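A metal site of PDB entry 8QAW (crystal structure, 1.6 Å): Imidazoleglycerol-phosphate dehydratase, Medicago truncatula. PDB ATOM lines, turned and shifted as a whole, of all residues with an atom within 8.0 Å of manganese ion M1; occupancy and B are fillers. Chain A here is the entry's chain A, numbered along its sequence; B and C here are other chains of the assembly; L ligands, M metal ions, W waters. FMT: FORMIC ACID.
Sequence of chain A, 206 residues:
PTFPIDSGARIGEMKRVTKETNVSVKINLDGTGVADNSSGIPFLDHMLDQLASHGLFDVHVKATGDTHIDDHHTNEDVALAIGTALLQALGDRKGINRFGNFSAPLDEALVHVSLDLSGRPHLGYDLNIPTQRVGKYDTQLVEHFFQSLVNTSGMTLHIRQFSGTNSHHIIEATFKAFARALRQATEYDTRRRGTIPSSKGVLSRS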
ATOM      1  N   HIS A  72     -22.072 -16.462   1.511  1.00  0.00           N
ATOM      2  CA  HIS A  72     -21.105 -17.461   1.980  1.00  0.00           C
ATOM      3  C   HIS A  72     -19.977 -17.690   0.983  1.00  0.00           C
ATOM      4  O   HIS A  72     -18.790 -17.627   1.345  1.00  0.00           O
ATOM      5  CB  HIS A  72     -21.835 -18.766   2.286  1.00  0.00           C
ATOM      6  CG  HIS A  72     -20.974 -19.811   2.928  1.00  0.00           C
ATOM      7  ND1 HIS A  72     -21.252 -20.326   4.176  1.00  0.00           N
ATOM      8  CD2 HIS A  72     -19.861 -20.448   2.501  1.00  0.00           C
ATOM      9  CE1 HIS A  72     -20.333 -21.234   4.488  1.00  0.00           C
ATOM     10  NE2 HIS A  72     -19.476 -21.319   3.491  1.00  0.00           N
ATOM     11  N   HIS A  73     -20.310 -17.985  -0.275  1.00  0.00           N
ATOM     12  CA  HIS A  73     -19.274 -18.327  -1.240  1.00  0.00           C
ATOM     13  C   HIS A  73     -18.358 -17.136  -1.488  1.00  0.00           C
ATOM     14  O   HIS A  73     -17.122 -17.289  -1.558  1.00  0.00           O
ATOM     15  CB  HIS A  73     -19.874 -18.822  -2.551  1.00  0.00           C
ATOM     16  CG  HIS A  73     -20.762 -20.031  -2.410  1.00  0.00           C
ATOM     17  ND1 HIS A  73     -21.714 -20.364  -3.351  1.00  0.00           N
ATOM     18  CD2 HIS A  73     -20.844 -20.960  -1.434  1.00  0.00           C
ATOM     19  CE1 HIS A  73     -22.356 -21.457  -2.948  1.00  0.00           C
ATOM     20  NE2 HIS A  73     -21.843 -21.841  -1.803  1.00  0.00           N
ATOM     21  N   ASN A  75     -17.755 -14.553   0.597  1.00  0.00           N
ATOM     22  CA  ASN A  75     -16.968 -14.376   1.816  1.00  0.00           C
ATOM     23  C   ASN A  75     -15.799 -15.354   1.864  1.00  0.00           C
ATOM     24  O   ASN A  75     -14.638 -14.955   2.107  1.00  0.00           O
ATOM     25  CB  ASN A  75     -17.907 -14.558   3.022  1.00  0.00           C
ATOM     26  CG  ASN A  75     -17.223 -14.303   4.350  1.00  0.00           C
ATOM     27  OD1 ASN A  75     -17.053 -13.153   4.759  1.00  0.00           O
ATOM     28  ND2 ASN A  75     -16.844 -15.370   5.041  1.00  0.00           N
ATOM     29  N   GLU A  76     -16.074 -16.624   1.588  1.00  0.00           N
ATOM     30  CA  GLU A  76     -15.064 -17.667   1.644  1.00  0.00           C
ATOM     31  C   GLU A  76     -13.993 -17.459   0.579  1.00  0.00           C
ATOM     32  O   GLU A  76     -12.794 -17.528   0.869  1.00  0.00           O
ATOM     33  CB  GLU A  76     -15.729 -19.033   1.466  1.00  0.00           C
ATOM     34  CG  GLU A  76     -14.751 -20.195   1.381  1.00  0.00           C
ATOM     35  CD  GLU A  76     -15.402 -21.552   1.659  1.00  0.00           C
ATOM     36  OE1 GLU A  76     -16.635 -21.638   1.884  1.00  0.00           O
ATOM     37  OE2 GLU A  76     -14.646 -22.559   1.659  1.00  0.00           O
ATOM     38  N   ASP A  77     -14.405 -17.208  -0.655  1.00  0.00           N
ATOM     39  CA  ASP A  77     -13.430 -17.106  -1.732  1.00  0.00           C
ATOM     40  C   ASP A  77     -12.578 -15.849  -1.615  1.00  0.00           C
ATOM     41  O   ASP A  77     -11.393 -15.856  -1.975  1.00  0.00           O
ATOM     42  CB  ASP A  77     -14.149 -17.173  -3.086  1.00  0.00           C
ATOM     43  CG  ASP A  77     -14.671 -18.581  -3.376  1.00  0.00           C
ATOM     44  OD1 ASP A  77     -14.301 -19.521  -2.637  1.00  0.00           O
ATOM     45  OD2 ASP A  77     -15.451 -18.743  -4.334  1.00  0.00           O
ATOM     46  N   LEU A  80     -10.011 -16.810   1.178  1.00  0.00           N
ATOM     47  CA  LEU A  80      -8.997 -17.703   0.608  1.00  0.00           C
ATOM     48  C   LEU A  80      -7.990 -16.931  -0.222  1.00  0.00           C
ATOM     49  O   LEU A  80      -6.782 -17.154  -0.116  1.00  0.00           O
ATOM     50  CB  LEU A  80      -9.663 -18.777  -0.256  1.00  0.00           C
ATOM     51  CG  LEU A  80     -10.525 -19.782   0.519  1.00  0.00           C
ATOM     52  CD1 LEU A  80     -11.344 -20.639  -0.446  1.00  0.00           C
ATOM     53  CD2 LEU A  80      -9.655 -20.650   1.401  1.00  0.00           C
ATOM     54  N   LEU A 141     -20.303 -15.617   9.203  1.00  0.00           N
ATOM     55  CA  LEU A 141     -19.260 -15.502   8.201  1.00  0.00           C
ATOM     56  C   LEU A 141     -17.951 -14.955   8.769  1.00  0.00           C
ATOM     57  O   LEU A 141     -16.928 -15.063   8.097  1.00  0.00           O
ATOM     58  CB  LEU A 141     -19.748 -14.621   7.049  1.00  0.00           C
ATOM     59  CG  LEU A 141     -20.956 -15.220   6.359  1.00  0.00           C
ATOM     60  CD1 LEU A 141     -21.446 -14.353   5.210  1.00  0.00           C
ATOM     61  CD2 LEU A 141     -20.619 -16.634   5.863  1.00  0.00           C
ATOM     62  N   HIS A 144     -15.748 -17.947   9.491  1.00  0.00           N
ATOM     63  CA  HIS A 144     -15.360 -18.588   8.241  1.00  0.00           C
ATOM     64  C   HIS A 144     -14.348 -17.745   7.481  1.00  0.00           C
ATOM     65  O   HIS A 144     -13.449 -18.292   6.818  1.00  0.00           O
ATOM     66  CB  HIS A 144     -16.600 -18.854   7.377  1.00  0.00           C
ATOM     67  CG  HIS A 144     -16.419 -19.940   6.349  1.00  0.00           C
ATOM     68  ND1 HIS A 144     -15.233 -20.122   5.661  1.00  0.00           N
ATOM     69  CD2 HIS A 144     -17.267 -20.891   5.912  1.00  0.00           C
ATOM     70  CE1 HIS A 144     -15.372 -21.141   4.833  1.00  0.00           C
ATOM     71  NE2 HIS A 144     -16.590 -21.627   4.960  1.00  0.00           N
ATOM     72  N   SER A 148     -10.767 -19.473   6.619  1.00  0.00           N
ATOM     73  CA  SER A 148     -10.298 -19.613   5.237  1.00  0.00           C
ATOM     74  C   SER A 148      -8.994 -18.860   5.016  1.00  0.00           C
ATOM     75  O   SER A 148      -8.090 -19.375   4.335  1.00  0.00           O
ATOM     76  CB  SER A 148     -11.370 -19.137   4.265  1.00  0.00           C
ATOM     77  OG  SER A 148     -12.515 -19.984   4.336  1.00  0.00           O
ATOM     78  N   LEU B 106     -18.593 -31.640   5.456  1.00  0.00           N
ATOM     79  CA  LEU B 106     -18.384 -30.364   4.770  1.00  0.00           C
ATOM     80  C   LEU B 106     -17.699 -29.485   5.798  1.00  0.00           C
ATOM     81  O   LEU B 106     -18.360 -28.930   6.693  1.00  0.00           O
ATOM     82  CB  LEU B 106     -19.680 -29.762   4.249  1.00  0.00           C
ATOM     83  CG  LEU B 106     -19.534 -28.729   3.106  1.00  0.00           C
ATOM     84  CD1 LEU B 106     -20.886 -28.191   2.661  1.00  0.00           C
ATOM     85  CD2 LEU B 106     -18.593 -27.564   3.439  1.00  0.00           C
ATOM     86  N   ASP B 107     -16.376 -29.368   5.679  1.00  0.00           N
ATOM     87  CA  ASP B 107     -15.567 -28.711   6.698  1.00  0.00           C
ATOM     88  C   ASP B 107     -15.933 -29.262   8.072  1.00  0.00           C
ATOM     89  O   ASP B 107     -15.819 -30.468   8.295  1.00  0.00           O
ATOM     90  CB  ASP B 107     -15.725 -27.200   6.591  1.00  0.00           C
ATOM     91  CG  ASP B 107     -15.144 -26.641   5.290  1.00  0.00           C
ATOM     92  OD1 ASP B 107     -14.580 -27.438   4.504  1.00  0.00           O
ATOM     93  OD2 ASP B 107     -15.254 -25.416   5.051  1.00  0.00           O
ATOM     94  N   GLU B 108     -16.383 -28.402   8.993  1.00  0.00           N
ATOM     95  CA  GLU B 108     -16.669 -28.864  10.355  1.00  0.00           C
ATOM     96  C   GLU B 108     -17.969 -29.647  10.461  1.00  0.00           C
ATOM     97  O   GLU B 108     -18.181 -30.332  11.483  1.00  0.00           O
ATOM     98  CB  GLU B 108     -16.700 -27.667  11.306  1.00  0.00           C
ATOM     99  CG  GLU B 108     -18.058 -27.016  11.536  1.00  0.00           C
ATOM    100  CD  GLU B 108     -18.688 -26.404  10.290  1.00  0.00           C
ATOM    101  OE1 GLU B 108     -17.984 -26.128   9.290  1.00  0.00           O
ATOM    102  OE2 GLU B 108     -19.923 -26.171  10.326  1.00  0.00           O
ATOM    103  N   ASN B 166     -21.822 -24.131  11.081  1.00  0.00           N
ATOM    104  CA  ASN B 166     -22.261 -23.202  10.058  1.00  0.00           C
ATOM    105  C   ASN B 166     -23.524 -23.745   9.392  1.00  0.00           C
ATOM    106  O   ASN B 166     -23.527 -24.880   8.907  1.00  0.00           O
ATOM    107  CB  ASN B 166     -21.135 -22.984   9.041  1.00  0.00           C
ATOM    108  CG  ASN B 166     -21.510 -22.011   7.952  1.00  0.00           C
ATOM    109  OD1 ASN B 166     -22.284 -22.329   7.057  1.00  0.00           O
ATOM    110  ND2 ASN B 166     -20.953 -20.792   8.013  1.00  0.00           N
ATOM    111  N   HIS B 168     -25.197 -23.008   6.597  1.00  0.00           N
ATOM    112  CA  HIS B 168     -25.000 -23.358   5.190  1.00  0.00           C
ATOM    113  C   HIS B 168     -24.247 -24.687   5.069  1.00  0.00           C
ATOM    114  O   HIS B 168     -24.643 -25.563   4.280  1.00  0.00           O
ATOM    115  CB  HIS B 168     -24.277 -22.176   4.519  1.00  0.00           C
ATOM    116  CG  HIS B 168     -24.100 -22.265   3.021  1.00  0.00           C
ATOM    117  ND1 HIS B 168     -24.235 -21.164   2.219  1.00  0.00           N
ATOM    118  CD2 HIS B 168     -23.709 -23.284   2.212  1.00  0.00           C
ATOM    119  CE1 HIS B 168     -23.948 -21.495   0.966  1.00  0.00           C
ATOM    120  NE2 HIS B 168     -23.639 -22.784   0.936  1.00  0.00           N
ATOM    121  N   HIS B 169     -23.188 -24.877   5.862  1.00  0.00           N
ATOM    122  CA  HIS B 169     -22.450 -26.151   5.825  1.00  0.00           C
ATOM    123  C   HIS B 169     -23.330 -27.321   6.236  1.00  0.00           C
ATOM    124  O   HIS B 169     -23.295 -28.375   5.602  1.00  0.00           O
ATOM    125  CB  HIS B 169     -21.208 -26.096   6.726  1.00  0.00           C
ATOM    126  CG  HIS B 169     -20.087 -25.270   6.171  1.00  0.00           C
ATOM    127  ND1 HIS B 169     -18.902 -25.055   6.853  1.00  0.00           N
ATOM    128  CD2 HIS B 169     -19.964 -24.604   4.995  1.00  0.00           C
ATOM    129  CE1 HIS B 169     -18.100 -24.289   6.118  1.00  0.00           C
ATOM    130  NE2 HIS B 169     -18.712 -24.015   4.975  1.00  0.00           N
ATOM    131  N   GLU B 172     -25.977 -28.000   3.472  1.00  0.00           N
ATOM    132  CA  GLU B 172     -25.363 -28.520   2.250  1.00  0.00           C
ATOM    133  C   GLU B 172     -24.818 -29.923   2.457  1.00  0.00           C
ATOM    134  O   GLU B 172     -24.956 -30.781   1.562  1.00  0.00           O
ATOM    135  CB  GLU B 172     -24.265 -27.568   1.763  1.00  0.00           C
ATOM    136  CG  GLU B 172     -23.708 -27.947   0.406  1.00  0.00           C
ATOM    137  CD  GLU B 172     -22.819 -26.872  -0.184  1.00  0.00           C
ATOM    138  OE1 GLU B 172     -23.048 -25.666   0.102  1.00  0.00           O
ATOM    139  OE2 GLU B 172     -21.911 -27.231  -0.956  1.00  0.00           O
ATOM    140  N   ARG C 120      -9.668 -28.268   1.353  1.00  0.00           N
ATOM    141  CA  ARG C 120      -9.822 -27.391   2.520  1.00  0.00           C
ATOM    142  C   ARG C 120      -9.440 -28.189   3.757  1.00  0.00           C
ATOM    143  O   ARG C 120     -10.133 -29.166   4.094  1.00  0.00           O
ATOM    144  CB  ARG C 120     -11.259 -26.882   2.639  1.00  0.00           C
ATOM    145  CG  ARG C 120     -11.752 -26.080   1.453  1.00  0.00           C
ATOM    146  CD  ARG C 120     -13.204 -25.625   1.657  1.00  0.00           C
ATOM    147  NE  ARG C 120     -14.115 -26.746   1.824  1.00  0.00           N
ATOM    148  CZ  ARG C 120     -14.691 -27.394   0.820  1.00  0.00           C
ATOM    149  NH1 ARG C 120     -14.464 -27.051  -0.447  1.00  0.00           N
ATOM    150  NH2 ARG C 120     -15.519 -28.403   1.088  1.00  0.00           N
HETATM  151  C   FMT L   1     -20.162 -23.643   1.410  1.00  0.00           C
HETATM  152  O1  FMT L   1     -20.587 -23.843   0.275  1.00  0.00           O
HETATM  153  O2  FMT L   1     -18.961 -23.715   1.722  1.00  0.00           O
HETATM  154 MN    MN M   1     -17.796 -22.801   3.352  1.00  0.00          MN
HETATM  155 MN    MN M   2     -22.536 -23.773  -0.825  1.00  0.00          MN
HETATM  156  O   HOH W   1     -16.211 -24.252   2.939  1.00  0.00           O
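OD1 of Asn 166 of chain B sits at hydrogen-bond distance from N of His 169 of chain B (3.0 Å). ND1 of His 169 of chain B lies within hydrogen-bond range of OE1 of Glu 108 of chain B (2.8 Å). ND1 of His 144 is in hydrogen-bond range of OG of Ser 148.
Of the 17 residues printed, 4 come within 4 Å of manganese ion M1.
Manganese ion M1 is bound by water W1 (2.2 Å). Manganese ion M1 is bound by O2 of the ligand, at 2.2 Å. The side-chain carboxylate (OE1) of Glu 76 is bound to manganese ion M1, 2.2 Å away. Manganese ion M1 is bound by NE2 of His 169 of chain B (2.2 Å). A ring nitrogen (NE2) of His 72 is bound to manganese ion M1, at 2.2 Å. Manganese ion M1 is bound by NE2 of His 144 (2.3 Å). Manganese ion M1 has six donor atoms within binding distance.
Water W1 lies within hydrogen-bond range of OD2 of Asp 107 of chain B (2.6 Å), OE2 of Glu 76 (2.6 Å) and NE of Arg 120 of chain C (3.4 Å).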
